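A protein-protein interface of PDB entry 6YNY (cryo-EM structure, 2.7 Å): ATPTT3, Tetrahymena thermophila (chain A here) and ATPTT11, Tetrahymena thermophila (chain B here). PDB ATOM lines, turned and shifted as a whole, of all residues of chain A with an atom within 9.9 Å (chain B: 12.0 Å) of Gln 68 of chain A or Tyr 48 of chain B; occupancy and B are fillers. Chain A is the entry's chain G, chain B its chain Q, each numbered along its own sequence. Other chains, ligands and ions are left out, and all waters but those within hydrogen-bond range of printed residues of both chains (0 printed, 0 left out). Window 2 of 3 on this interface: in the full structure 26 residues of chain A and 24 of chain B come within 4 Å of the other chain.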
ATOM      1  N   ARG A  57      15.868 -26.941   0.259  1.00  0.00           N
ATOM      2  CA  ARG A  57      16.539 -25.728   0.711  1.00  0.00           C
ATOM      3  C   ARG A  57      15.895 -25.183   1.975  1.00  0.00           C
ATOM      4  O   ARG A  57      16.578 -24.902   2.966  1.00  0.00           O
ATOM      5  CB  ARG A  57      16.503 -24.678  -0.395  1.00  0.00           C
ATOM      6  CG  ARG A  57      17.298 -23.430  -0.095  1.00  0.00           C
ATOM      7  CD  ARG A  57      17.031 -22.366  -1.124  1.00  0.00           C
ATOM      8  NE  ARG A  57      15.646 -21.922  -1.082  1.00  0.00           N
ATOM      9  CZ  ARG A  57      15.103 -21.095  -1.964  1.00  0.00           C
ATOM     10  NH1 ARG A  57      13.833 -20.746  -1.846  1.00  0.00           N
ATOM     11  NH2 ARG A  57      15.825 -20.618  -2.962  1.00  0.00           N
ATOM     12  N   ASP A  58      14.578 -25.024   1.957  1.00  0.00           N
ATOM     13  CA  ASP A  58      13.832 -24.496   3.084  1.00  0.00           C
ATOM     14  C   ASP A  58      12.798 -25.514   3.531  1.00  0.00           C
ATOM     15  O   ASP A  58      12.331 -26.337   2.740  1.00  0.00           O
ATOM     16  CB  ASP A  58      13.134 -23.184   2.715  1.00  0.00           C
ATOM     17  CG  ASP A  58      14.060 -22.199   2.035  1.00  0.00           C
ATOM     18  OD1 ASP A  58      15.266 -22.192   2.355  1.00  0.00           O
ATOM     19  OD2 ASP A  58      13.582 -21.431   1.175  1.00  0.00           O
ATOM     20  N   HIS A  61       6.853 -24.642   3.375  1.00  0.00           N
ATOM     21  CA  HIS A  61       6.280 -23.334   3.639  1.00  0.00           C
ATOM     22  C   HIS A  61       4.832 -23.458   4.086  1.00  0.00           C
ATOM     23  O   HIS A  61       4.051 -24.224   3.516  1.00  0.00           O
ATOM     24  CB  HIS A  61       6.364 -22.456   2.393  1.00  0.00           C
ATOM     25  CG  HIS A  61       7.760 -22.108   1.990  1.00  0.00           C
ATOM     26  ND1 HIS A  61       8.848 -22.335   2.803  1.00  0.00           N
ATOM     27  CD2 HIS A  61       8.247 -21.544   0.860  1.00  0.00           C
ATOM     28  CE1 HIS A  61       9.945 -21.928   2.190  1.00  0.00           C
ATOM     29  NE2 HIS A  61       9.607 -21.444   1.010  1.00  0.00           N
ATOM     30  N   VAL A  64       2.638 -18.597   1.173  1.00  0.00           N
ATOM     31  CA  VAL A  64       3.435 -18.099   0.062  1.00  0.00           C
ATOM     32  C   VAL A  64       4.331 -16.975   0.560  1.00  0.00           C
ATOM     33  O   VAL A  64       3.874 -16.046   1.237  1.00  0.00           O
ATOM     34  CB  VAL A  64       2.529 -17.629  -1.083  1.00  0.00           C
ATOM     35  CG1 VAL A  64       3.357 -17.082  -2.220  1.00  0.00           C
ATOM     36  CG2 VAL A  64       1.664 -18.768  -1.562  1.00  0.00           C
ATOM     37  N   ARG A  65       5.612 -17.058   0.230  1.00  0.00           N
ATOM     38  CA  ARG A  65       6.620 -16.127   0.704  1.00  0.00           C
ATOM     39  C   ARG A  65       7.183 -15.326  -0.462  1.00  0.00           C
ATOM     40  O   ARG A  65       6.782 -15.487  -1.616  1.00  0.00           O
ATOM     41  CB  ARG A  65       7.725 -16.880   1.442  1.00  0.00           C
ATOM     42  CG  ARG A  65       7.223 -17.646   2.645  1.00  0.00           C
ATOM     43  CD  ARG A  65       8.312 -18.446   3.315  1.00  0.00           C
ATOM     44  NE  ARG A  65       7.771 -19.276   4.382  1.00  0.00           N
ATOM     45  CZ  ARG A  65       8.499 -20.083   5.143  1.00  0.00           C
ATOM     46  NH1 ARG A  65       7.912 -20.801   6.088  1.00  0.00           N
ATOM     47  NH2 ARG A  65       9.809 -20.169   4.964  1.00  0.00           N
ATOM     48  N   LYS A  66       8.115 -14.449  -0.144  1.00  0.00           N
ATOM     49  CA  LYS A  66       8.750 -13.586  -1.118  1.00  0.00           C
ATOM     50  C   LYS A  66      10.128 -14.111  -1.484  1.00  0.00           C
ATOM     51  O   LYS A  66      10.750 -14.848  -0.714  1.00  0.00           O
ATOM     52  CB  LYS A  66       8.870 -12.166  -0.565  1.00  0.00           C
ATOM     53  CG  LYS A  66       7.560 -11.583  -0.095  1.00  0.00           C
ATOM     54  CD  LYS A  66       7.715 -10.175   0.438  1.00  0.00           C
ATOM     55  CE  LYS A  66       8.577 -10.124   1.685  1.00  0.00           C
ATOM     56  NZ  LYS A  66       8.066 -10.997   2.767  1.00  0.00           N
ATOM     57  N   PRO A  67      10.640 -13.751  -2.662  1.00  0.00           N
ATOM     58  CA  PRO A  67      11.976 -14.227  -3.047  1.00  0.00           C
ATOM     59  C   PRO A  67      13.057 -13.860  -2.051  1.00  0.00           C
ATOM     60  O   PRO A  67      14.008 -14.629  -1.870  1.00  0.00           O
ATOM     61  CB  PRO A  67      12.206 -13.551  -4.403  1.00  0.00           C
ATOM     62  CG  PRO A  67      10.854 -13.265  -4.919  1.00  0.00           C
ATOM     63  CD  PRO A  67      10.014 -12.957  -3.730  1.00  0.00           C
ATOM     64  N   GLN A  68      12.941 -12.706  -1.400  1.00  0.00           N
ATOM     65  CA  GLN A  68      13.929 -12.287  -0.417  1.00  0.00           C
ATOM     66  C   GLN A  68      13.706 -12.914   0.951  1.00  0.00           C
ATOM     67  O   GLN A  68      14.576 -12.787   1.818  1.00  0.00           O
ATOM     68  CB  GLN A  68      13.934 -10.762  -0.291  1.00  0.00           C
ATOM     69  CG  GLN A  68      12.581 -10.136  -0.013  1.00  0.00           C
ATOM     70  CD  GLN A  68      11.830  -9.782  -1.279  1.00  0.00           C
ATOM     71  OE1 GLN A  68      12.073 -10.356  -2.338  1.00  0.00           O
ATOM     72  NE2 GLN A  68      10.919  -8.828  -1.176  1.00  0.00           N
ATOM     73  N   ASP A  69      12.573 -13.584   1.167  1.00  0.00           N
ATOM     74  CA  ASP A  69      12.357 -14.269   2.435  1.00  0.00           C
ATOM     75  C   ASP A  69      13.282 -15.468   2.579  1.00  0.00           C
ATOM     76  O   ASP A  69      13.659 -15.828   3.698  1.00  0.00           O
ATOM     77  CB  ASP A  69      10.900 -14.707   2.557  1.00  0.00           C
ATOM     78  CG  ASP A  69       9.945 -13.538   2.628  1.00  0.00           C
ATOM     79  OD1 ASP A  69      10.372 -12.444   3.047  1.00  0.00           O
ATOM     80  OD2 ASP A  69       8.761 -13.713   2.270  1.00  0.00           O
ATOM     81  N   SER A  70      13.647 -16.095   1.468  1.00  0.00           N
ATOM     82  CA  SER A  70      14.572 -17.216   1.455  1.00  0.00           C
ATOM     83  C   SER A  70      15.953 -16.750   1.010  1.00  0.00           C
ATOM     84  O   SER A  70      16.149 -15.612   0.578  1.00  0.00           O
ATOM     85  CB  SER A  70      14.060 -18.330   0.541  1.00  0.00           C
ATOM     86  OG  SER A  70      13.844 -17.851  -0.769  1.00  0.00           O
ATOM     87  N   LYS A  71      16.916 -17.656   1.118  1.00  0.00           N
ATOM     88  CA  LYS A  71      18.313 -17.373   0.817  1.00  0.00           C
ATOM     89  C   LYS A  71      18.724 -18.166  -0.416  1.00  0.00           C
ATOM     90  O   LYS A  71      18.834 -19.395  -0.362  1.00  0.00           O
ATOM     91  CB  LYS A  71      19.190 -17.719   2.017  1.00  0.00           C
ATOM     92  CG  LYS A  71      20.670 -17.521   1.799  1.00  0.00           C
ATOM     93  CD  LYS A  71      21.428 -17.529   3.117  1.00  0.00           C
ATOM     94  CE  LYS A  71      21.151 -18.785   3.924  1.00  0.00           C
ATOM     95  NZ  LYS A  71      22.004 -18.868   5.144  1.00  0.00           N
ATOM     96  N   ASP A  72      18.950 -17.462  -1.522  1.00  0.00           N
ATOM     97  CA  ASP A  72      19.440 -18.103  -2.729  1.00  0.00           C
ATOM     98  C   ASP A  72      20.822 -18.698  -2.486  1.00  0.00           C
ATOM     99  O   ASP A  72      21.550 -18.290  -1.577  1.00  0.00           O
ATOM    100  CB  ASP A  72      19.502 -17.099  -3.876  1.00  0.00           C
ATOM    101  CG  ASP A  72      18.164 -16.447  -4.155  1.00  0.00           C
ATOM    102  OD1 ASP A  72      17.124 -17.113  -3.973  1.00  0.00           O
ATOM    103  OD2 ASP A  72      18.153 -15.264  -4.557  1.00  0.00           O
ATOM    104  N   LEU B  45       5.110 -11.295   7.117  1.00  0.00           N
ATOM    105  CA  LEU B  45       3.658 -11.176   7.069  1.00  0.00           C
ATOM    106  C   LEU B  45       3.217 -10.409   5.828  1.00  0.00           C
ATOM    107  O   LEU B  45       2.068  -9.980   5.731  1.00  0.00           O
ATOM    108  CB  LEU B  45       3.131 -10.477   8.322  1.00  0.00           C
ATOM    109  CG  LEU B  45       3.449 -11.124   9.671  1.00  0.00           C
ATOM    110  CD1 LEU B  45       4.901 -10.890  10.070  1.00  0.00           C
ATOM    111  CD2 LEU B  45       2.512 -10.601  10.746  1.00  0.00           C
ATOM    112  N   THR B  46       4.136 -10.235   4.885  1.00  0.00           N
ATOM    113  CA  THR B  46       3.884  -9.492   3.661  1.00  0.00           C
ATOM    114  C   THR B  46       3.947 -10.422   2.458  1.00  0.00           C
ATOM    115  O   THR B  46       4.619 -11.456   2.484  1.00  0.00           O
ATOM    116  CB  THR B  46       4.896  -8.359   3.483  1.00  0.00           C
ATOM    117  OG1 THR B  46       6.225  -8.895   3.480  1.00  0.00           O
ATOM    118  CG2 THR B  46       4.762  -7.350   4.602  1.00  0.00           C
ATOM    119  N   GLN B  47       3.236 -10.040   1.402  1.00  0.00           N
ATOM    120  CA  GLN B  47       3.208 -10.807   0.169  1.00  0.00           C
ATOM    121  C   GLN B  47       3.180  -9.860  -1.019  1.00  0.00           C
ATOM    122  O   GLN B  47       2.689  -8.732  -0.925  1.00  0.00           O
ATOM    123  CB  GLN B  47       1.993 -11.735   0.104  1.00  0.00           C
ATOM    124  CG  GLN B  47       1.965 -12.812   1.164  1.00  0.00           C
ATOM    125  CD  GLN B  47       0.837 -13.796   0.951  1.00  0.00           C
ATOM    126  OE1 GLN B  47      -0.042 -13.579   0.117  1.00  0.00           O
ATOM    127  NE2 GLN B  47       0.857 -14.890   1.699  1.00  0.00           N
ATOM    128  N   TYR B  48       3.714 -10.333  -2.139  1.00  0.00           N
ATOM    129  CA  TYR B  48       3.634  -9.594  -3.387  1.00  0.00           C
ATOM    130  C   TYR B  48       2.250  -9.762  -3.995  1.00  0.00           C
ATOM    131  O   TYR B  48       1.704 -10.867  -4.037  1.00  0.00           O
ATOM    132  CB  TYR B  48       4.695 -10.079  -4.373  1.00  0.00           C
ATOM    133  CG  TYR B  48       6.063  -9.481  -4.168  1.00  0.00           C
ATOM    134  CD1 TYR B  48       6.990 -10.092  -3.344  1.00  0.00           C
ATOM    135  CD2 TYR B  48       6.430  -8.310  -4.810  1.00  0.00           C
ATOM    136  CE1 TYR B  48       8.241  -9.551  -3.159  1.00  0.00           C
ATOM    137  CE2 TYR B  48       7.678  -7.762  -4.629  1.00  0.00           C
ATOM    138  CZ  TYR B  48       8.580  -8.387  -3.803  1.00  0.00           C
ATOM    139  OH  TYR B  48       9.827  -7.842  -3.621  1.00  0.00           O
ATOM    140  N   VAL B  49       1.680  -8.654  -4.458  1.00  0.00           N
ATOM    141  CA  VAL B  49       0.378  -8.645  -5.113  1.00  0.00           C
ATOM    142  C   VAL B  49       0.532  -7.804  -6.373  1.00  0.00           C
ATOM    143  O   VAL B  49       0.552  -6.571  -6.306  1.00  0.00           O
ATOM    144  CB  VAL B  49      -0.729  -8.098  -4.212  1.00  0.00           C
ATOM    145  CG1 VAL B  49      -2.049  -8.118  -4.938  1.00  0.00           C
ATOM    146  CG2 VAL B  49      -0.821  -8.914  -2.948  1.00  0.00           C
ATOM    147  N   GLU B  50       0.645  -8.467  -7.523  1.00  0.00           N
ATOM    148  CA  GLU B  50       0.821  -7.786  -8.802  1.00  0.00           C
ATOM    149  C   GLU B  50       2.080  -6.925  -8.799  1.00  0.00           C
ATOM    150  O   GLU B  50       2.091  -5.805  -9.312  1.00  0.00           O
ATOM    151  CB  GLU B  50      -0.410  -6.950  -9.148  1.00  0.00           C
ATOM    152  CG  GLU B  50      -1.669  -7.771  -9.339  1.00  0.00           C
ATOM    153  CD  GLU B  50      -1.592  -8.692 -10.542  1.00  0.00           C
ATOM    154  OE1 GLU B  50      -0.718  -8.472 -11.406  1.00  0.00           O
ATOM    155  OE2 GLU B  50      -2.401  -9.638 -10.622  1.00  0.00           O
ATOM    156  N   GLY B  51       3.152  -7.454  -8.214  1.00  0.00           N
ATOM    157  CA  GLY B  51       4.425  -6.774  -8.180  1.00  0.00           C
ATOM    158  C   GLY B  51       4.609  -5.815  -7.029  1.00  0.00           C
ATOM    159  O   GLY B  51       5.719  -5.298  -6.849  1.00  0.00           O
ATOM    160  N   GLN B  52       3.569  -5.560  -6.244  1.00  0.00           N
ATOM    161  CA  GLN B  52       3.637  -4.648  -5.117  1.00  0.00           C
ATOM    162  C   GLN B  52       3.543  -5.424  -3.812  1.00  0.00           C
ATOM    163  O   GLN B  52       2.733  -6.346  -3.682  1.00  0.00           O
ATOM    164  CB  GLN B  52       2.515  -3.611  -5.183  1.00  0.00           C
ATOM    165  CG  GLN B  52       2.550  -2.740  -6.422  1.00  0.00           C
ATOM    166  CD  GLN B  52       3.798  -1.885  -6.499  1.00  0.00           C
ATOM    167  OE1 GLN B  52       4.523  -1.735  -5.518  1.00  0.00           O
ATOM    168  NE2 GLN B  52       4.054  -1.320  -7.672  1.00  0.00           N
ATOM    169  N   ILE B  53       4.381  -5.047  -2.854  1.00  0.00           N
ATOM    170  CA  ILE B  53       4.369  -5.668  -1.536  1.00  0.00           C
ATOM    171  C   ILE B  53       3.184  -5.130  -0.748  1.00  0.00           C
ATOM    172  O   ILE B  53       2.941  -3.918  -0.717  1.00  0.00           O
ATOM    173  CB  ILE B  53       5.691  -5.407  -0.800  1.00  0.00           C
ATOM    174  CG1 ILE B  53       6.837  -6.110  -1.523  1.00  0.00           C
ATOM    175  CG2 ILE B  53       5.595  -5.875   0.640  1.00  0.00           C
ATOM    176  CD1 ILE B  53       8.204  -5.750  -0.999  1.00  0.00           C
ATOM    177  N   VAL B  54       2.444  -6.032  -0.113  1.00  0.00           N
ATOM    178  CA  VAL B  54       1.258  -5.681   0.656  1.00  0.00           C
ATOM    179  C   VAL B  54       1.280  -6.457   1.964  1.00  0.00           C
ATOM    180  O   VAL B  54       1.711  -7.614   2.006  1.00  0.00           O
ATOM    181  CB  VAL B  54      -0.032  -5.978  -0.131  1.00  0.00           C
ATOM    182  CG1 VAL B  54      -1.250  -5.536   0.658  1.00  0.00           C
ATOM    183  CG2 VAL B  54       0.011  -5.296  -1.479  1.00  0.00           C
ATOM    184  N   ASN B  55       0.817  -5.816   3.031  1.00  0.00           N
ATOM    185  CA  ASN B  55       0.734  -6.468   4.328  1.00  0.00           C
ATOM    186  C   ASN B  55      -0.477  -7.391   4.365  1.00  0.00           C
ATOM    187  O   ASN B  55      -1.591  -6.984   4.024  1.00  0.00           O
ATOM    188  CB  ASN B  55       0.648  -5.431   5.446  1.00  0.00           C
ATOM    189  CG  ASN B  55       0.515  -6.063   6.814  1.00  0.00           C
ATOM    190  OD1 ASN B  55      -0.585  -6.183   7.351  1.00  0.00           O
ATOM    191  ND2 ASN B  55       1.640  -6.481   7.386  1.00  0.00           N
ATOM    192  N   ARG B  56      -0.251  -8.633   4.776  1.00  0.00           N
ATOM    193  CA  ARG B  56      -1.312  -9.625   4.826  1.00  0.00           C
ATOM    194  C   ARG B  56      -2.124  -9.474   6.104  1.00  0.00           C
ATOM    195  O   ARG B  56      -1.585  -9.148   7.166  1.00  0.00           O
ATOM    196  CB  ARG B  56      -0.724 -11.033   4.741  1.00  0.00           C
ATOM    197  CG  ARG B  56      -1.764 -12.133   4.664  1.00  0.00           C
ATOM    198  CD  ARG B  56      -1.131 -13.512   4.674  1.00  0.00           C
ATOM    199  NE  ARG B  56      -0.335 -13.745   5.875  1.00  0.00           N
ATOM    200  CZ  ARG B  56       0.075 -14.943   6.278  1.00  0.00           C
ATOM    201  NH1 ARG B  56       0.798 -15.061   7.382  1.00  0.00           N
ATOM    202  NH2 ARG B  56      -0.247 -16.026   5.587  1.00  0.00           N
ATOM    203  N   ASN B  57      -3.426  -9.715   5.997  1.00  0.00           N
ATOM    204  CA  ASN B  57      -4.345  -9.625   7.120  1.00  0.00           C
ATOM    205  C   ASN B  57      -4.898 -11.003   7.459  1.00  0.00           C
ATOM    206  O   ASN B  57      -5.227 -11.789   6.565  1.00  0.00           O
ATOM    207  CB  ASN B  57      -5.496  -8.666   6.809  1.00  0.00           C
ATOM    208  CG  ASN B  57      -6.177  -8.978   5.491  1.00  0.00           C
ATOM    209  OD1 ASN B  57      -5.957 -10.035   4.898  1.00  0.00           O
ATOM    210  ND2 ASN B  57      -7.010  -8.058   5.025  1.00  0.00           N
ATOM    211  N   GLN B 109      -5.319 -21.778   0.569  1.00  0.00           N
ATOM    212  CA  GLN B 109      -5.781 -20.408   0.709  1.00  0.00           C
ATOM    213  C   GLN B 109      -6.417 -20.160   2.067  1.00  0.00           C
ATOM    214  O   GLN B 109      -6.448 -19.014   2.525  1.00  0.00           O
ATOM    215  CB  GLN B 109      -6.776 -20.081  -0.402  1.00  0.00           C
ATOM    216  CG  GLN B 109      -7.138 -18.618  -0.509  1.00  0.00           C
ATOM    217  CD  GLN B 109      -5.981 -17.766  -0.979  1.00  0.00           C
ATOM    218  OE1 GLN B 109      -4.986 -18.276  -1.490  1.00  0.00           O
ATOM    219  NE2 GLN B 109      -6.107 -16.460  -0.807  1.00  0.00           N
ATOM    220  N   GLU B 112      -3.706 -19.210   4.346  1.00  0.00           N
ATOM    221  CA  GLU B 112      -3.267 -17.840   4.115  1.00  0.00           C
ATOM    222  C   GLU B 112      -4.157 -16.847   4.849  1.00  0.00           C
ATOM    223  O   GLU B 112      -3.663 -15.870   5.423  1.00  0.00           O
ATOM    224  CB  GLU B 112      -3.270 -17.541   2.616  1.00  0.00           C
ATOM    225  CG  GLU B 112      -2.315 -18.390   1.799  1.00  0.00           C
ATOM    226  CD  GLU B 112      -0.886 -17.894   1.855  1.00  0.00           C
ATOM    227  OE1 GLU B 112      -0.655 -16.783   2.378  1.00  0.00           O
ATOM    228  OE2 GLU B 112       0.011 -18.614   1.371  1.00  0.00           O
ATOM    229  N   ASP B 113      -5.465 -17.083   4.847  1.00  0.00           N
ATOM    230  CA  ASP B 113      -6.418 -16.125   5.389  1.00  0.00           C
ATOM    231  C   ASP B 113      -6.611 -16.272   6.893  1.00  0.00           C
ATOM    232  O   ASP B 113      -6.763 -15.269   7.596  1.00  0.00           O
ATOM    233  CB  ASP B 113      -7.764 -16.282   4.685  1.00  0.00           C
ATOM    234  CG  ASP B 113      -7.667 -16.078   3.187  1.00  0.00           C
ATOM    235  OD1 ASP B 113      -6.822 -15.272   2.747  1.00  0.00           O
ATOM    236  OD2 ASP B 113      -8.436 -16.725   2.447  1.00  0.00           O
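NE2 of Gln 47 of chain B sits at hydrogen-bond distance from OE1 of Glu 112 of chain B, at 2.5 Å.
The backbone NH of Val 54 of chain B lies within hydrogen-bond range of the backbone carbonyl oxygen of Gln 47 of chain B (2.8 Å).
The guanidinium group (NH2) of Arg 56 of chain B is in salt-bridge range of the side-chain carboxylate (OE1) of Glu 112 of chain B, at 3.3 Å.
O of Pro 67 of chain A sits at hydrogen-bond distance from OG of Ser 70 of chain A.
NZ of Lys 66 of chain A is in salt-bridge range of OD1 of Asp 69 of chain A (2.7 Å).
His 61 of chain A touches none of the printed residues of chain B.
Of the printed residues of chain B, Val 64 of chain A touches Gln 47 and Glu 112.
No residue of chain B comes within 4 Å of Asp 69 of chain A.
Of the printed residues of chain A, Thr 46 of chain B touches Lys 66.
Of the printed residues of chain A, Gln 47 of chain B touches Val 64.
Of chain A, only Lys 66, Pro 67 and Gln 68 come within 4 Å of Tyr 48 of chain B.
Val 49 of chain B touches none of the printed residues of chain A.
Gly 51 of chain B touches none of the printed residues of chain A.
Asn 57 of chain B touches none of the printed residues of chain A.
The nearest residue of chain B that does not touch Gln 68 of chain A is Ile 53 of chain B (4.1 Å).
The nearest residue of chain A that does not touch Tyr 48 of chain B is Arg 65 of chain A (5.7 Å).
Hydrophobic or aromatic side chains of chain B within 4 Å of the printed part of chain A: Tyr 48.
Among the printed residues, pairs that only touch across the chains: Lys 66 of chain A with Tyr 48 of chain B (3.6 Å) and Pro 67 of chain A with Tyr 48 of chain B (3.9 Å).
OG1 of Thr 46 of chain B sits at hydrogen-bond distance from NZ of Lys 66 of chain A (2.9 Å).
The side-chain amide nitrogen of Gln 47 of chain B sits at hydrogen-bond distance from the backbone carbonyl oxygen of Val 64 of chain A (3.3 Å).
OE2 of Glu 112 of chain B sits at hydrogen-bond distance from N of Val 64 of chain A (2.6 Å).
OH of Tyr 48 of chain B sits at hydrogen-bond distance from NE2 of Gln 68 of chain A (2.9 Å).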
